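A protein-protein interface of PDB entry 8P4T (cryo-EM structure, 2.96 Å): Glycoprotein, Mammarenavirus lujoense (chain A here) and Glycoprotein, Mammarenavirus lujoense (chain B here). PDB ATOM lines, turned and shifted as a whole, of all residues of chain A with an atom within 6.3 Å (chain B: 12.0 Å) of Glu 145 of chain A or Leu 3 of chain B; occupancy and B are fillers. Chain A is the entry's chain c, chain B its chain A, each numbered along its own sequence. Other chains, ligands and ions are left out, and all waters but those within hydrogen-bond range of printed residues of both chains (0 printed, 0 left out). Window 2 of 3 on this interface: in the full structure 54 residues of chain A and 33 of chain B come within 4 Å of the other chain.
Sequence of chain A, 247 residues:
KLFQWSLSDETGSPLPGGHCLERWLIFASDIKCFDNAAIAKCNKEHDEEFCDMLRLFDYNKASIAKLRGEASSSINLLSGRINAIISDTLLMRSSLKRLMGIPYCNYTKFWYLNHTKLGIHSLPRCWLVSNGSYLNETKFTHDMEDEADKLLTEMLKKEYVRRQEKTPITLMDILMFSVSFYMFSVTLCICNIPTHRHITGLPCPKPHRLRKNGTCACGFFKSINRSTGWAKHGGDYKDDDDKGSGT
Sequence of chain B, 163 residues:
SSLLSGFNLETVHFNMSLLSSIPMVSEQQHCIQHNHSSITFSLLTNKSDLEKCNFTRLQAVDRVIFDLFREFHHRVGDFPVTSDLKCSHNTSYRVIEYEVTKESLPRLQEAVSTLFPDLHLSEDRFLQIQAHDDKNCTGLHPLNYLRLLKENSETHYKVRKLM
Among the printed residues, merely in contact across the chains: Leu 113 of chain A with Leu 4 of chain B (3.6 Å), Leu 113 of chain A with Asn 8 of chain B (3.2 Å), Leu 113 of chain A with Leu 9 of chain B (3.6 Å), Thr 141 of chain A with Leu 4 of chain B (3.8 Å), Met 144 of chain A with Leu 4 of chain B (3.7 Å), Met 144 of chain A with Leu 9 of chain B (3.7 Å), Glu 145 of chain A with Ser 2 of chain B (3.9 Å), Glu 145 of chain A with Leu 3 of chain B (3.6 Å), Ala 148 of chain A with Phe 7 of chain B (3.6 Å), Asp 149 of chain A with Leu 3 of chain B (3.8 Å) and Leu 152 of chain A with Phe 7 of chain B (3.5 Å).
Thr 141 of chain A touches one residue of chain B.
No residue of chain B comes within 4 Å of Asp 143 of chain A.
Of chain B, only Leu 4 and Leu 9 come within 4 Å of Met 144 of chain A.
No residue of chain B comes within 4 Å of Asp 146 of chain A.
Of the printed residues of chain B, Ala 148 of chain A touches Phe 7.
Of the printed residues of chain A, Ser 2 of chain B touches Glu 145 (3.9 Å).
Printed residues of chain A within 4 Å of Leu 3 of chain B: Glu 145 and Asp 149.
The nearest residue of chain B that does not touch Glu 145 of chain A is Leu 4 of chain B (4.2 Å).
The nearest printed residue of chain A that does not touch Leu 3 of chain B is Ala 148 of chain A (4.02 Å).
The nearest printed residue of chain A that does not touch Leu 9 of chain B is Phe 140 of chain A (4.3 Å).
Of the 13 printed residues of chain A, 7 touch a printed residue of chain B.
Of the 8 printed residues of chain B, 6 touch a printed residue of chain A.
Hydrophobic or aromatic side chains of chain B within 4 Å of the printed part of chain A: Leu 3, Leu 4, Phe 7 and Leu 9.
Among the printed residues, 11 pairs touch across the chains.
Among the printed residues, no Asp or Glu carboxylate lies within 4 Å of a Lys or Arg side-chain nitrogen of the other chain.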
ATOM      1  N   LEU A 113      -4.908  -5.249 -10.304  1.00  0.00           N
ATOM      2  CA  LEU A 113      -4.598  -3.991  -9.627  1.00  0.00           C
ATOM      3  C   LEU A 113      -5.038  -2.817 -10.496  1.00  0.00           C
ATOM      4  O   LEU A 113      -4.473  -2.581 -11.567  1.00  0.00           O
ATOM      5  CB  LEU A 113      -3.106  -3.907  -9.319  1.00  0.00           C
ATOM      6  CG  LEU A 113      -2.563  -4.931  -8.325  1.00  0.00           C
ATOM      7  CD1 LEU A 113      -1.069  -4.742  -8.130  1.00  0.00           C
ATOM      8  CD2 LEU A 113      -3.299  -4.823  -7.002  1.00  0.00           C
ATOM      9  N   PHE A 140      -0.287 -13.617  -0.862  1.00  0.00           N
ATOM     10  CA  PHE A 140       0.248 -13.344  -2.191  1.00  0.00           C
ATOM     11  C   PHE A 140       0.570 -11.865  -2.386  1.00  0.00           C
ATOM     12  O   PHE A 140       0.720 -11.417  -3.526  1.00  0.00           O
ATOM     13  CB  PHE A 140      -0.706 -13.844  -3.283  1.00  0.00           C
ATOM     14  CG  PHE A 140      -2.009 -13.100  -3.351  1.00  0.00           C
ATOM     15  CD1 PHE A 140      -3.082 -13.491  -2.570  1.00  0.00           C
ATOM     16  CD2 PHE A 140      -2.171 -12.030  -4.215  1.00  0.00           C
ATOM     17  CE1 PHE A 140      -4.282 -12.816  -2.638  1.00  0.00           C
ATOM     18  CE2 PHE A 140      -3.368 -11.351  -4.283  1.00  0.00           C
ATOM     19  CZ  PHE A 140      -4.424 -11.745  -3.494  1.00  0.00           C
ATOM     20  N   THR A 141       0.688 -11.099  -1.297  1.00  0.00           N
ATOM     21  CA  THR A 141       0.989  -9.675  -1.413  1.00  0.00           C
ATOM     22  C   THR A 141       2.343  -9.421  -2.064  1.00  0.00           C
ATOM     23  O   THR A 141       2.556  -8.338  -2.624  1.00  0.00           O
ATOM     24  CB  THR A 141       0.937  -9.010  -0.036  1.00  0.00           C
ATOM     25  OG1 THR A 141       1.212  -7.610  -0.168  1.00  0.00           O
ATOM     26  CG2 THR A 141       1.959  -9.635   0.902  1.00  0.00           C
ATOM     27  N   HIS A 142       3.253 -10.396  -2.020  1.00  0.00           N
ATOM     28  CA  HIS A 142       4.482 -10.286  -2.795  1.00  0.00           C
ATOM     29  C   HIS A 142       4.176 -10.263  -4.286  1.00  0.00           C
ATOM     30  O   HIS A 142       4.779  -9.494  -5.043  1.00  0.00           O
ATOM     31  CB  HIS A 142       5.424 -11.440  -2.454  1.00  0.00           C
ATOM     32  CG  HIS A 142       6.575 -11.582  -3.400  1.00  0.00           C
ATOM     33  ND1 HIS A 142       7.605 -10.667  -3.461  1.00  0.00           N
ATOM     34  CD2 HIS A 142       6.861 -12.531  -4.322  1.00  0.00           C
ATOM     35  CE1 HIS A 142       8.475 -11.048  -4.380  1.00  0.00           C
ATOM     36  NE2 HIS A 142       8.047 -12.175  -4.917  1.00  0.00           N
ATOM     37  N   ASP A 143       3.223 -11.091  -4.723  1.00  0.00           N
ATOM     38  CA  ASP A 143       2.786 -11.051  -6.114  1.00  0.00           C
ATOM     39  C   ASP A 143       2.139  -9.714  -6.449  1.00  0.00           C
ATOM     40  O   ASP A 143       2.311  -9.197  -7.555  1.00  0.00           O
ATOM     41  CB  ASP A 143       1.819 -12.200  -6.398  1.00  0.00           C
ATOM     42  CG  ASP A 143       2.489 -13.557  -6.327  1.00  0.00           C
ATOM     43  OD1 ASP A 143       3.705 -13.637  -6.602  1.00  0.00           O
ATOM     44  OD2 ASP A 143       1.800 -14.545  -5.998  1.00  0.00           O
ATOM     45  N   MET A 144       1.386  -9.139  -5.508  1.00  0.00           N
ATOM     46  CA  MET A 144       0.774  -7.834  -5.749  1.00  0.00           C
ATOM     47  C   MET A 144       1.828  -6.742  -5.911  1.00  0.00           C
ATOM     48  O   MET A 144       1.717  -5.886  -6.798  1.00  0.00           O
ATOM     49  CB  MET A 144      -0.187  -7.491  -4.611  1.00  0.00           C
ATOM     50  CG  MET A 144      -1.564  -8.118  -4.752  1.00  0.00           C
ATOM     51  SD  MET A 144      -2.766  -7.437  -3.593  1.00  0.00           S
ATOM     52  CE  MET A 144      -2.440  -8.431  -2.141  1.00  0.00           C
ATOM     53  N   GLU A 145       2.861  -6.755  -5.064  1.00  0.00           N
ATOM     54  CA  GLU A 145       3.938  -5.776  -5.203  1.00  0.00           C
ATOM     55  C   GLU A 145       4.697  -5.975  -6.510  1.00  0.00           C
ATOM     56  O   GLU A 145       5.043  -5.000  -7.197  1.00  0.00           O
ATOM     57  CB  GLU A 145       4.885  -5.869  -4.006  1.00  0.00           C
ATOM     58  CG  GLU A 145       6.226  -5.185  -4.211  1.00  0.00           C
ATOM     59  CD  GLU A 145       6.204  -3.728  -3.797  1.00  0.00           C
ATOM     60  OE1 GLU A 145       5.299  -3.341  -3.027  1.00  0.00           O
ATOM     61  OE2 GLU A 145       7.091  -2.968  -4.240  1.00  0.00           O
ATOM     62  N   ASP A 146       4.958  -7.235  -6.873  1.00  0.00           N
ATOM     63  CA  ASP A 146       5.602  -7.521  -8.149  1.00  0.00           C
ATOM     64  C   ASP A 146       4.754  -7.024  -9.310  1.00  0.00           C
ATOM     65  O   ASP A 146       5.285  -6.498 -10.291  1.00  0.00           O
ATOM     66  CB  ASP A 146       5.863  -9.021  -8.285  1.00  0.00           C
ATOM     67  CG  ASP A 146       6.960  -9.508  -7.360  1.00  0.00           C
ATOM     68  OD1 ASP A 146       7.824  -8.691  -6.978  1.00  0.00           O
ATOM     69  OD2 ASP A 146       6.960 -10.709  -7.020  1.00  0.00           O
ATOM     70  N   GLU A 147       3.431  -7.163  -9.208  1.00  0.00           N
ATOM     71  CA  GLU A 147       2.555  -6.719 -10.285  1.00  0.00           C
ATOM     72  C   GLU A 147       2.471  -5.202 -10.355  1.00  0.00           C
ATOM     73  O   GLU A 147       2.312  -4.649 -11.443  1.00  0.00           O
ATOM     74  CB  GLU A 147       1.161  -7.322 -10.112  1.00  0.00           C
ATOM     75  CG  GLU A 147       0.369  -7.435 -11.405  1.00  0.00           C
ATOM     76  CD  GLU A 147       0.870  -8.549 -12.304  1.00  0.00           C
ATOM     77  OE1 GLU A 147       1.625  -9.416 -11.818  1.00  0.00           O
ATOM     78  OE2 GLU A 147       0.508  -8.556 -13.499  1.00  0.00           O
ATOM     79  N   ALA A 148       2.603  -4.511  -9.223  1.00  0.00           N
ATOM     80  CA  ALA A 148       2.637  -3.049  -9.262  1.00  0.00           C
ATOM     81  C   ALA A 148       3.922  -2.545  -9.917  1.00  0.00           C
ATOM     82  O   ALA A 148       3.892  -1.654 -10.786  1.00  0.00           O
ATOM     83  CB  ALA A 148       2.495  -2.487  -7.848  1.00  0.00           C
ATOM     84  N   ASP A 149       5.064  -3.113  -9.518  1.00  0.00           N
ATOM     85  CA  ASP A 149       6.321  -2.757 -10.171  1.00  0.00           C
ATOM     86  C   ASP A 149       6.283  -3.108 -11.654  1.00  0.00           C
ATOM     87  O   ASP A 149       6.771  -2.343 -12.497  1.00  0.00           O
ATOM     88  CB  ASP A 149       7.488  -3.463  -9.480  1.00  0.00           C
ATOM     89  CG  ASP A 149       8.821  -3.173 -10.142  1.00  0.00           C
ATOM     90  OD1 ASP A 149       9.000  -2.048 -10.656  1.00  0.00           O
ATOM     91  OD2 ASP A 149       9.689  -4.070 -10.149  1.00  0.00           O
ATOM     92  N   LYS A 150       5.695  -4.260 -11.986  1.00  0.00           N
ATOM     93  CA  LYS A 150       5.519  -4.646 -13.379  1.00  0.00           C
ATOM     94  C   LYS A 150       4.632  -3.656 -14.115  1.00  0.00           C
ATOM     95  O   LYS A 150       4.877  -3.354 -15.282  1.00  0.00           O
ATOM     96  CB  LYS A 150       4.936  -6.057 -13.458  1.00  0.00           C
ATOM     97  CG  LYS A 150       4.962  -6.667 -14.848  1.00  0.00           C
ATOM     98  CD  LYS A 150       4.214  -7.989 -14.879  1.00  0.00           C
ATOM     99  CE  LYS A 150       4.914  -9.036 -14.028  1.00  0.00           C
ATOM    100  NZ  LYS A 150       4.181 -10.331 -14.021  1.00  0.00           N
ATOM    101  N   LEU A 152       4.278  -0.390 -13.532  1.00  0.00           N
ATOM    102  CA  LEU A 152       5.054   0.814 -13.843  1.00  0.00           C
ATOM    103  C   LEU A 152       6.063   0.553 -14.963  1.00  0.00           C
ATOM    104  O   LEU A 152       6.120   1.291 -15.966  1.00  0.00           O
ATOM    105  CB  LEU A 152       5.765   1.331 -12.589  1.00  0.00           C
ATOM    106  CG  LEU A 152       4.998   2.219 -11.601  1.00  0.00           C
ATOM    107  CD1 LEU A 152       4.596   3.529 -12.265  1.00  0.00           C
ATOM    108  CD2 LEU A 152       3.782   1.525 -11.010  1.00  0.00           C
ATOM    109  N   SER B   2       3.841   1.484   0.591  1.00  0.00           N
ATOM    110  CA  SER B   2       4.545   0.780  -0.475  1.00  0.00           C
ATOM    111  C   SER B   2       3.949   1.111  -1.838  1.00  0.00           C
ATOM    112  O   SER B   2       3.130   2.022  -1.964  1.00  0.00           O
ATOM    113  CB  SER B   2       4.505  -0.732  -0.237  1.00  0.00           C
ATOM    114  OG  SER B   2       5.059  -1.066   1.024  1.00  0.00           O
ATOM    115  N   LEU B   3       4.375   0.366  -2.861  1.00  0.00           N
ATOM    116  CA  LEU B   3       3.811   0.546  -4.195  1.00  0.00           C
ATOM    117  C   LEU B   3       2.332   0.180  -4.223  1.00  0.00           C
ATOM    118  O   LEU B   3       1.531   0.847  -4.886  1.00  0.00           O
ATOM    119  CB  LEU B   3       4.589  -0.292  -5.211  1.00  0.00           C
ATOM    120  CG  LEU B   3       5.771   0.383  -5.912  1.00  0.00           C
ATOM    121  CD1 LEU B   3       6.948   0.543  -4.962  1.00  0.00           C
ATOM    122  CD2 LEU B   3       6.179  -0.403  -7.148  1.00  0.00           C
ATOM    123  N   LEU B   4       1.952  -0.876  -3.501  1.00  0.00           N
ATOM    124  CA  LEU B   4       0.585  -1.382  -3.522  1.00  0.00           C
ATOM    125  C   LEU B   4      -0.406  -0.452  -2.831  1.00  0.00           C
ATOM    126  O   LEU B   4      -1.618  -0.640  -2.987  1.00  0.00           O
ATOM    127  CB  LEU B   4       0.553  -2.769  -2.873  1.00  0.00           C
ATOM    128  CG  LEU B   4      -0.743  -3.581  -2.881  1.00  0.00           C
ATOM    129  CD1 LEU B   4      -1.142  -3.922  -4.304  1.00  0.00           C
ATOM    130  CD2 LEU B   4      -0.595  -4.841  -2.043  1.00  0.00           C
ATOM    131  N   SER B   5       0.072   0.552  -2.093  1.00  0.00           N
ATOM    132  CA  SER B   5      -0.834   1.473  -1.412  1.00  0.00           C
ATOM    133  C   SER B   5      -1.675   2.267  -2.405  1.00  0.00           C
ATOM    134  O   SER B   5      -2.889   2.417  -2.227  1.00  0.00           O
ATOM    135  CB  SER B   5      -0.036   2.414  -0.509  1.00  0.00           C
ATOM    136  OG  SER B   5      -0.819   3.524  -0.108  1.00  0.00           O
ATOM    137  N   GLY B   6      -1.045   2.789  -3.458  1.00  0.00           N
ATOM    138  CA  GLY B   6      -1.798   3.504  -4.477  1.00  0.00           C
ATOM    139  C   GLY B   6      -2.739   2.616  -5.270  1.00  0.00           C
ATOM    140  O   GLY B   6      -3.861   3.016  -5.592  1.00  0.00           O
ATOM    141  N   PHE B   7      -2.300   1.403  -5.600  1.00  0.00           N
ATOM    142  CA  PHE B   7      -3.118   0.497  -6.393  1.00  0.00           C
ATOM    143  C   PHE B   7      -4.252  -0.100  -5.565  1.00  0.00           C
ATOM    144  O   PHE B   7      -4.156  -0.250  -4.344  1.00  0.00           O
ATOM    145  CB  PHE B   7      -2.254  -0.621  -6.976  1.00  0.00           C
ATOM    146  CG  PHE B   7      -1.240  -0.141  -7.971  1.00  0.00           C
ATOM    147  CD1 PHE B   7      -1.555  -0.057  -9.316  1.00  0.00           C
ATOM    148  CD2 PHE B   7       0.027   0.237  -7.562  1.00  0.00           C
ATOM    149  CE1 PHE B   7      -0.625   0.386 -10.233  1.00  0.00           C
ATOM    150  CE2 PHE B   7       0.960   0.683  -8.475  1.00  0.00           C
ATOM    151  CZ  PHE B   7       0.634   0.756  -9.812  1.00  0.00           C
ATOM    152  N   ASN B   8      -5.342  -0.440  -6.252  1.00  0.00           N
ATOM    153  CA  ASN B   8      -6.519  -1.041  -5.642  1.00  0.00           C
ATOM    154  C   ASN B   8      -6.710  -2.453  -6.183  1.00  0.00           C
ATOM    155  O   ASN B   8      -6.440  -2.717  -7.358  1.00  0.00           O
ATOM    156  CB  ASN B   8      -7.771  -0.202  -5.915  1.00  0.00           C
ATOM    157  CG  ASN B   8      -8.819  -0.349  -4.832  1.00  0.00           C
ATOM    158  OD1 ASN B   8      -8.634  -1.096  -3.871  1.00  0.00           O
ATOM    159  ND2 ASN B   8      -9.929   0.364  -4.981  1.00  0.00           N
ATOM    160  N   LEU B   9      -7.177  -3.354  -5.323  1.00  0.00           N
ATOM    161  CA  LEU B   9      -7.448  -4.735  -5.706  1.00  0.00           C
ATOM    162  C   LEU B   9      -8.895  -4.865  -6.170  1.00  0.00           C
ATOM    163  O   LEU B   9      -9.823  -4.581  -5.406  1.00  0.00           O
ATOM    164  CB  LEU B   9      -7.171  -5.680  -4.538  1.00  0.00           C
ATOM    165  CG  LEU B   9      -6.872  -7.139  -4.884  1.00  0.00           C
ATOM    166  CD1 LEU B   9      -5.805  -7.225  -5.961  1.00  0.00           C
ATOM    167  CD2 LEU B   9      -6.447  -7.904  -3.643  1.00  0.00           C
